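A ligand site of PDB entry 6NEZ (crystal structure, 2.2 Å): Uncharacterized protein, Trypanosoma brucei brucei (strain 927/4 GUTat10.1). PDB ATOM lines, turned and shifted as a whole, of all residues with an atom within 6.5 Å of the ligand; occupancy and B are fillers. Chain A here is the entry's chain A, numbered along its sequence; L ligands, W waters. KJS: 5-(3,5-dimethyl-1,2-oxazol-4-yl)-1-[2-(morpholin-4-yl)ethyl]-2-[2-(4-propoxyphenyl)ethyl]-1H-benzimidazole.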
ATOM      1  N   GLU A  26     -11.058  -2.053   9.806  1.00  0.00           N
ATOM      2  CA  GLU A  26     -11.028  -0.966   8.780  1.00  0.00           C
ATOM      3  C   GLU A  26     -10.100   0.185   9.204  1.00  0.00           C
ATOM      4  O   GLU A  26      -9.876   1.100   8.355  1.00  0.00           O
ATOM      5  CB  GLU A  26     -12.433  -0.426   8.510  1.00  0.00           C
ATOM      6  CG  GLU A  26     -13.144  -1.150   7.383  1.00  0.00           C
ATOM      7  CD  GLU A  26     -13.749  -2.482   7.754  1.00  0.00           C
ATOM      8  OE1 GLU A  26     -13.479  -3.479   7.071  1.00  0.00           O
ATOM      9  OE2 GLU A  26     -14.491  -2.507   8.728  1.00  0.00           O
ATOM     10  N   ASN A  27      -9.586   0.151  10.435  1.00  0.00           N
ATOM     11  CA  ASN A  27      -8.595   1.135  10.965  1.00  0.00           C
ATOM     12  C   ASN A  27      -9.130   2.555  10.738  1.00  0.00           C
ATOM     13  O   ASN A  27      -8.329   3.426  10.356  1.00  0.00           O
ATOM     14  CB  ASN A  27      -7.203   0.949  10.322  1.00  0.00           C
ATOM     15  CG  ASN A  27      -6.608  -0.440  10.481  1.00  0.00           C
ATOM     16  OD1 ASN A  27      -5.970  -0.950   9.555  1.00  0.00           O
ATOM     17  ND2 ASN A  27      -6.789  -1.060  11.630  1.00  0.00           N
ATOM     18  N   GLY A  28     -10.431   2.789  10.974  1.00  0.00           N
ATOM     19  CA  GLY A  28     -11.059   4.125  10.936  1.00  0.00           C
ATOM     20  C   GLY A  28     -11.361   4.634   9.519  1.00  0.00           C
ATOM     21  O   GLY A  28     -11.710   5.834   9.380  1.00  0.00           O
ATOM     22  N   LEU A  29     -11.255   3.786   8.502  1.00  0.00           N
ATOM     23  CA  LEU A  29     -11.444   4.229   7.096  1.00  0.00           C
ATOM     24  C   LEU A  29     -12.791   4.939   6.913  1.00  0.00           C
ATOM     25  O   LEU A  29     -12.813   5.950   6.219  1.00  0.00           O
ATOM     26  CB  LEU A  29     -11.313   3.031   6.160  1.00  0.00           C
ATOM     27  CG  LEU A  29     -11.232   3.367   4.675  1.00  0.00           C
ATOM     28  CD1 LEU A  29     -10.211   4.487   4.402  1.00  0.00           C
ATOM     29  CD2 LEU A  29     -10.904   2.134   3.861  1.00  0.00           C
ATOM     30  N   PHE A  30     -13.880   4.457   7.508  1.00  0.00           N
ATOM     31  CA  PHE A  30     -15.234   5.025   7.234  1.00  0.00           C
ATOM     32  C   PHE A  30     -15.813   5.667   8.498  1.00  0.00           C
ATOM     33  O   PHE A  30     -16.991   6.035   8.455  1.00  0.00           O
ATOM     34  CB  PHE A  30     -16.161   3.936   6.675  1.00  0.00           C
ATOM     35  CG  PHE A  30     -15.716   3.405   5.341  1.00  0.00           C
ATOM     36  CD1 PHE A  30     -15.766   4.209   4.212  1.00  0.00           C
ATOM     37  CD2 PHE A  30     -15.222   2.125   5.213  1.00  0.00           C
ATOM     38  CE1 PHE A  30     -15.355   3.731   2.971  1.00  0.00           C
ATOM     39  CE2 PHE A  30     -14.802   1.650   3.977  1.00  0.00           C
ATOM     40  CZ  PHE A  30     -14.860   2.451   2.865  1.00  0.00           C
ATOM     41  N   SER A  31     -15.027   5.801   9.571  1.00  0.00           N
ATOM     42  CA  SER A  31     -15.513   6.275  10.887  1.00  0.00           C
ATOM     43  C   SER A  31     -16.102   7.687  10.768  1.00  0.00           C
ATOM     44  O   SER A  31     -17.115   7.944  11.411  1.00  0.00           O
ATOM     45  CB  SER A  31     -14.444   6.212  11.942  1.00  0.00           C
ATOM     46  OG  SER A  31     -13.996   4.876  12.073  1.00  0.00           O
ATOM     47  N   GLN A  32     -15.487   8.572   9.987  1.00  0.00           N
ATOM     48  CA  GLN A  32     -15.796  10.012  10.038  1.00  0.00           C
ATOM     49  C   GLN A  32     -15.731  10.661   8.660  1.00  0.00           C
ATOM     50  O   GLN A  32     -15.060  10.111   7.766  1.00  0.00           O
ATOM     51  CB  GLN A  32     -14.809  10.703  10.978  1.00  0.00           C
ATOM     52  CG  GLN A  32     -14.964  10.267  12.424  1.00  0.00           C
ATOM     53  CD  GLN A  32     -14.226  11.167  13.379  1.00  0.00           C
ATOM     54  OE1 GLN A  32     -14.439  12.376  13.406  1.00  0.00           O
ATOM     55  NE2 GLN A  32     -13.347  10.567  14.172  1.00  0.00           N
ATOM     56  N   VAL A  34     -14.771  12.672   5.534  1.00  0.00           N
ATOM     57  CA  VAL A  34     -13.436  12.848   4.886  1.00  0.00           C
ATOM     58  C   VAL A  34     -12.935  14.279   5.117  1.00  0.00           C
ATOM     59  O   VAL A  34     -11.769  14.432   5.502  1.00  0.00           O
ATOM     60  CB  VAL A  34     -13.529  12.506   3.383  1.00  0.00           C
ATOM     61  CG1 VAL A  34     -12.275  12.938   2.624  1.00  0.00           C
ATOM     62  CG2 VAL A  34     -13.804  11.027   3.162  1.00  0.00           C
ATOM     63  N   GLN A  37     -11.826  15.319   8.781  1.00  0.00           N
ATOM     64  CA  GLN A  37     -10.505  14.709   9.079  1.00  0.00           C
ATOM     65  C   GLN A  37      -9.386  15.335   8.240  1.00  0.00           C
ATOM     66  O   GLN A  37      -8.247  15.363   8.761  1.00  0.00           O
ATOM     67  CB  GLN A  37     -10.492  13.233   8.692  1.00  0.00           C
ATOM     68  CG  GLN A  37     -11.037  12.314   9.769  1.00  0.00           C
ATOM     69  CD  GLN A  37     -11.266  10.941   9.184  1.00  0.00           C
ATOM     70  OE1 GLN A  37     -10.523  10.009   9.471  1.00  0.00           O
ATOM     71  NE2 GLN A  37     -12.289  10.812   8.356  1.00  0.00           N
ATOM     72  N   TYR A  38      -9.665  15.685   6.978  1.00  0.00           N
ATOM     73  CA  TYR A  38      -8.650  16.145   5.976  1.00  0.00           C
ATOM     74  C   TYR A  38      -9.113  17.424   5.282  1.00  0.00           C
ATOM     75  O   TYR A  38      -9.432  17.432   4.105  1.00  0.00           O
ATOM     76  CB  TYR A  38      -8.368  15.042   4.959  1.00  0.00           C
ATOM     77  CG  TYR A  38      -7.997  13.729   5.582  1.00  0.00           C
ATOM     78  CD1 TYR A  38      -6.883  13.604   6.413  1.00  0.00           C
ATOM     79  CD2 TYR A  38      -8.767  12.605   5.359  1.00  0.00           C
ATOM     80  CE1 TYR A  38      -6.566  12.388   7.004  1.00  0.00           C
ATOM     81  CE2 TYR A  38      -8.466  11.394   5.954  1.00  0.00           C
ATOM     82  CZ  TYR A  38      -7.372  11.284   6.790  1.00  0.00           C
ATOM     83  OH  TYR A  38      -7.086  10.035   7.304  1.00  0.00           O
ATOM     84  N   LEU A  41      -8.658  18.643   1.562  1.00  0.00           N
ATOM     85  CA  LEU A  41      -9.357  17.966   0.425  1.00  0.00           C
ATOM     86  C   LEU A  41     -10.667  18.665   0.068  1.00  0.00           C
ATOM     87  O   LEU A  41     -11.365  18.109  -0.748  1.00  0.00           O
ATOM     88  CB  LEU A  41      -9.680  16.521   0.789  1.00  0.00           C
ATOM     89  CG  LEU A  41      -8.483  15.644   1.122  1.00  0.00           C
ATOM     90  CD1 LEU A  41      -8.917  14.189   1.320  1.00  0.00           C
ATOM     91  CD2 LEU A  41      -7.430  15.756   0.040  1.00  0.00           C
ATOM     92  N   TYR A  45     -11.700  16.513  -3.137  1.00  0.00           N
ATOM     93  CA  TYR A  45     -12.638  15.412  -2.833  1.00  0.00           C
ATOM     94  C   TYR A  45     -14.029  15.718  -3.421  1.00  0.00           C
ATOM     95  O   TYR A  45     -14.581  14.845  -4.094  1.00  0.00           O
ATOM     96  CB  TYR A  45     -12.678  15.134  -1.330  1.00  0.00           C
ATOM     97  CG  TYR A  45     -13.448  13.892  -0.979  1.00  0.00           C
ATOM     98  CD1 TYR A  45     -12.952  12.620  -1.273  1.00  0.00           C
ATOM     99  CD2 TYR A  45     -14.708  13.975  -0.401  1.00  0.00           C
ATOM    100  CE1 TYR A  45     -13.672  11.479  -0.972  1.00  0.00           C
ATOM    101  CE2 TYR A  45     -15.441  12.840  -0.105  1.00  0.00           C
ATOM    102  CZ  TYR A  45     -14.922  11.598  -0.372  1.00  0.00           C
ATOM    103  OH  TYR A  45     -15.658  10.516  -0.037  1.00  0.00           O
ATOM    104  N   MET A  83     -20.451   5.652   0.653  1.00  0.00           N
ATOM    105  CA  MET A  83     -19.124   5.568   1.346  1.00  0.00           C
ATOM    106  C   MET A  83     -18.156   4.752   0.496  1.00  0.00           C
ATOM    107  O   MET A  83     -17.021   5.203   0.286  1.00  0.00           O
ATOM    108  CB  MET A  83     -19.205   4.828   2.680  1.00  0.00           C
ATOM    109  CG  MET A  83     -19.751   5.606   3.768  1.00  0.00           C
ATOM    110  SD  MET A  83     -19.924   4.548   5.223  1.00  0.00           S
ATOM    111  CE  MET A  83     -21.412   5.315   5.853  1.00  0.00           C
ATOM    112  N   ASN A  86     -17.440   6.064  -3.220  1.00  0.00           N
ATOM    113  CA  ASN A  86     -16.587   7.289  -3.155  1.00  0.00           C
ATOM    114  C   ASN A  86     -15.136   6.850  -2.904  1.00  0.00           C
ATOM    115  O   ASN A  86     -14.238   7.294  -3.629  1.00  0.00           O
ATOM    116  CB  ASN A  86     -17.051   8.265  -2.065  1.00  0.00           C
ATOM    117  CG  ASN A  86     -18.290   9.085  -2.414  1.00  0.00           C
ATOM    118  OD1 ASN A  86     -18.793   9.049  -3.529  1.00  0.00           O
ATOM    119  ND2 ASN A  86     -18.789   9.834  -1.464  1.00  0.00           N
ATOM    120  N   CYS A  87     -14.908   6.023  -1.895  1.00  0.00           N
ATOM    121  CA  CYS A  87     -13.568   5.537  -1.514  1.00  0.00           C
ATOM    122  C   CYS A  87     -12.897   4.928  -2.752  1.00  0.00           C
ATOM    123  O   CYS A  87     -11.725   5.274  -3.005  1.00  0.00           O
ATOM    124  CB  CYS A  87     -13.638   4.521  -0.373  1.00  0.00           C
ATOM    125  SG  CYS A  87     -11.994   4.050   0.232  1.00  0.00           S
ATOM    126  N   PHE A  90     -12.337   7.777  -5.605  1.00  0.00           N
ATOM    127  CA  PHE A  90     -11.333   8.806  -5.219  1.00  0.00           C
ATOM    128  C   PHE A  90      -9.925   8.191  -5.127  1.00  0.00           C
ATOM    129  O   PHE A  90      -8.991   8.832  -5.582  1.00  0.00           O
ATOM    130  CB  PHE A  90     -11.696   9.482  -3.914  1.00  0.00           C
ATOM    131  CG  PHE A  90     -10.842  10.679  -3.585  1.00  0.00           C
ATOM    132  CD1 PHE A  90     -10.803  11.773  -4.428  1.00  0.00           C
ATOM    133  CD2 PHE A  90     -10.085  10.709  -2.430  1.00  0.00           C
ATOM    134  CE1 PHE A  90     -10.031  12.878  -4.107  1.00  0.00           C
ATOM    135  CE2 PHE A  90      -9.316  11.823  -2.109  1.00  0.00           C
ATOM    136  CZ  PHE A  90      -9.303  12.908  -2.943  1.00  0.00           C
ATOM    137  N   ASN A  91      -9.779   6.977  -4.595  1.00  0.00           N
ATOM    138  CA  ASN A  91      -8.442   6.360  -4.369  1.00  0.00           C
ATOM    139  C   ASN A  91      -7.986   5.517  -5.577  1.00  0.00           C
ATOM    140  O   ASN A  91      -6.771   5.245  -5.647  1.00  0.00           O
ATOM    141  CB  ASN A  91      -8.424   5.569  -3.074  1.00  0.00           C
ATOM    142  CG  ASN A  91      -8.683   6.460  -1.889  1.00  0.00           C
ATOM    143  OD1 ASN A  91      -7.879   7.342  -1.609  1.00  0.00           O
ATOM    144  ND2 ASN A  91      -9.808   6.254  -1.213  1.00  0.00           N
ATOM    145  N   ALA A  96      -5.381  -0.321  -2.833  1.00  0.00           N
ATOM    146  CA  ALA A  96      -5.588  -0.947  -1.496  1.00  0.00           C
ATOM    147  C   ALA A  96      -6.783  -0.308  -0.770  1.00  0.00           C
ATOM    148  O   ALA A  96      -7.501  -1.050  -0.072  1.00  0.00           O
ATOM    149  CB  ALA A  96      -4.296  -0.850  -0.681  1.00  0.00           C
ATOM    150  N   TYR A  97      -7.017   0.997  -0.905  1.00  0.00           N
ATOM    151  CA  TYR A  97      -8.191   1.694  -0.304  1.00  0.00           C
ATOM    152  C   TYR A  97      -9.486   1.101  -0.884  1.00  0.00           C
ATOM    153  O   TYR A  97     -10.417   0.868  -0.132  1.00  0.00           O
ATOM    154  CB  TYR A  97      -8.116   3.213  -0.496  1.00  0.00           C
ATOM    155  CG  TYR A  97      -7.280   3.958   0.515  1.00  0.00           C
ATOM    156  CD1 TYR A  97      -7.682   4.059   1.837  1.00  0.00           C
ATOM    157  CD2 TYR A  97      -6.097   4.594   0.178  1.00  0.00           C
ATOM    158  CE1 TYR A  97      -6.936   4.750   2.786  1.00  0.00           C
ATOM    159  CE2 TYR A  97      -5.342   5.298   1.099  1.00  0.00           C
ATOM    160  CZ  TYR A  97      -5.770   5.379   2.417  1.00  0.00           C
ATOM    161  OH  TYR A  97      -5.057   6.069   3.361  1.00  0.00           O
ATOM    162  N   ALA A  98      -9.540   0.839  -2.200  1.00  0.00           N
ATOM    163  CA  ALA A  98     -10.656   0.139  -2.868  1.00  0.00           C
ATOM    164  C   ALA A  98     -10.799  -1.293  -2.338  1.00  0.00           C
ATOM    165  O   ALA A  98     -11.929  -1.688  -2.062  1.00  0.00           O
ATOM    166  CB  ALA A  98     -10.468   0.130  -4.366  1.00  0.00           C
ATOM    167  N   ASP A  99      -9.706  -2.050  -2.160  1.00  0.00           N
ATOM    168  CA  ASP A  99      -9.777  -3.414  -1.564  1.00  0.00           C
ATOM    169  C   ASP A  99     -10.481  -3.302  -0.194  1.00  0.00           C
ATOM    170  O   ASP A  99     -11.424  -4.056   0.061  1.00  0.00           O
ATOM    171  CB  ASP A  99      -8.403  -4.082  -1.395  1.00  0.00           C
ATOM    172  CG  ASP A  99      -7.706  -4.481  -2.690  1.00  0.00           C
ATOM    173  OD1 ASP A  99      -8.390  -4.526  -3.746  1.00  0.00           O
ATOM    174  OD2 ASP A  99      -6.461  -4.730  -2.652  1.00  0.00           O
ATOM    175  N   ALA A 100     -10.012  -2.382   0.649  1.00  0.00           N
ATOM    176  CA  ALA A 100     -10.523  -2.171   2.013  1.00  0.00           C
ATOM    177  C   ALA A 100     -12.013  -1.807   1.934  1.00  0.00           C
ATOM    178  O   ALA A 100     -12.812  -2.343   2.713  1.00  0.00           O
ATOM    179  CB  ALA A 100      -9.675  -1.140   2.716  1.00  0.00           C
HETATM  180  C4  KJS L   1      -4.461   3.108   5.493  1.00  0.00           C
HETATM  181  C5  KJS L   1      -4.523   3.940   6.595  1.00  0.00           C
HETATM  182  C6  KJS L   1      -5.688   4.049   7.333  1.00  0.00           C
HETATM  183  N1  KJS L   1      -8.074   7.114   7.688  1.00  0.00           N
HETATM  184  C7  KJS L   1      -5.769   5.013   8.491  1.00  0.00           C
HETATM  185  C8  KJS L   1      -5.679   6.459   8.051  1.00  0.00           C
HETATM  186  N2  KJS L   1      -8.474   8.130  11.282  1.00  0.00           N
HETATM  187  C9  KJS L   1      -6.822   6.881   7.184  1.00  0.00           C
HETATM  188  C10 KJS L   1      -8.012   7.443   5.501  1.00  0.00           C
HETATM  189  C11 KJS L   1      -8.503   7.803   4.251  1.00  0.00           C
HETATM  190  C12 KJS L   1      -9.828   8.224   4.135  1.00  0.00           C
HETATM  191  N3  KJS L   1     -10.532   9.410   0.745  1.00  0.00           N
HETATM  192  C13 KJS L   1     -10.656   8.267   5.269  1.00  0.00           C
HETATM  193  C14 KJS L   1     -10.191   7.887   6.514  1.00  0.00           C
HETATM  194  C15 KJS L   1      -8.859   7.489   6.603  1.00  0.00           C
HETATM  195  C26 KJS L   1      -8.716  10.441   1.973  1.00  0.00           C
HETATM  196  C25 KJS L   1      -9.866   9.492   1.854  1.00  0.00           C
HETATM  197  O2  KJS L   1     -11.547   8.429   0.954  1.00  0.00           O
HETATM  198  C23 KJS L   1     -11.420   7.962   2.204  1.00  0.00           C
HETATM  199  C24 KJS L   1     -12.413   6.950   2.641  1.00  0.00           C
HETATM  200  C22 KJS L   1     -10.380   8.593   2.814  1.00  0.00           C
HETATM  201  N   KJS L   1      -6.734   7.052   5.889  1.00  0.00           N
HETATM  202  C16 KJS L   1      -8.551   7.041   9.070  1.00  0.00           C
HETATM  203  C17 KJS L   1      -8.159   8.273   9.867  1.00  0.00           C
HETATM  204  C21 KJS L   1      -7.410   7.380  11.961  1.00  0.00           C
HETATM  205  C20 KJS L   1      -7.726   7.238  13.421  1.00  0.00           C
HETATM  206  O1  KJS L   1      -7.930   8.522  14.055  1.00  0.00           O
HETATM  207  C19 KJS L   1      -8.932   9.271  13.372  1.00  0.00           C
HETATM  208  C18 KJS L   1      -8.607   9.439  11.921  1.00  0.00           C
HETATM  209  C27 KJS L   1      -6.754   3.222   7.016  1.00  0.00           C
HETATM  210  C28 KJS L   1      -6.690   2.359   5.933  1.00  0.00           C
HETATM  211  C3  KJS L   1      -5.568   2.372   5.125  1.00  0.00           C
HETATM  212  O   KJS L   1      -5.326   1.729   3.936  1.00  0.00           O
HETATM  213  C2  KJS L   1      -6.307   0.823   3.402  1.00  0.00           C
HETATM  214  C1  KJS L   1      -5.539  -0.295   2.712  1.00  0.00           C
HETATM  215  C   KJS L   1      -4.803  -1.229   3.688  1.00  0.00           C
HETATM  216  O   HOH W   1     -14.451   8.386  -0.058  1.00  0.00           O
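Asn 27 touches the ligand (O to C7, 3.5 Å). Gly 28 touches the ligand (O to C16, 3.4 Å). Leu 29 touches the ligand. CG2 of Val 34 touches C23 of the ligand (3.999 Å). CD1 of Leu 41 touches C26 of the ligand, 3.8 Å away. Cys 87 touches the ligand (SG to C24, 3.8 Å). Phe 90 touches the ligand. ND2 of Asn 91 touches O2 of the ligand, at 3.5 Å. O of Ala 96 touches C1 of the ligand (3.5 Å). Ala 100 touches the ligand. Of the 22 residues printed, 13 come within 4 Å of the ligand. Along chain A the residues within 4 Å of the ligand span positions 27 to 100. The nearest printed residue that does not touch the ligand is Glu 26 (4.01 Å).
The side-chain sulfur of Cys 87 sits at hydrogen-bond distance from the backbone carbonyl oxygen of Tyr 97 (3.6 Å). The backbone carbonyl oxygen (O) of Gln 32 is in hydrogen-bond range of the side-chain amide nitrogen (NE2) of Gln 37, at 2.9 Å. The backbone carbonyl oxygen of Cys 87 lies within hydrogen-bond range of the side-chain amide nitrogen of Asn 91.
The side-chain hydroxyl (OH) of Tyr 38 sits close to a nitrogen (N) of the ligand (3.3 Å). OE1 of Gln 37 lies close to N2 of the ligand, 3.3 Å away. The side-chain hydroxyl (OH) of Tyr 97 sits at hydrogen-bond distance from a nitrogen (N) of the ligand, 3.2 Å away.
Water W1 lies within hydrogen-bond range of the side-chain hydroxyl (OH) of Tyr 45, the backbone NH (N) of Cys 87 and an oxygen (O2) of the ligand.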
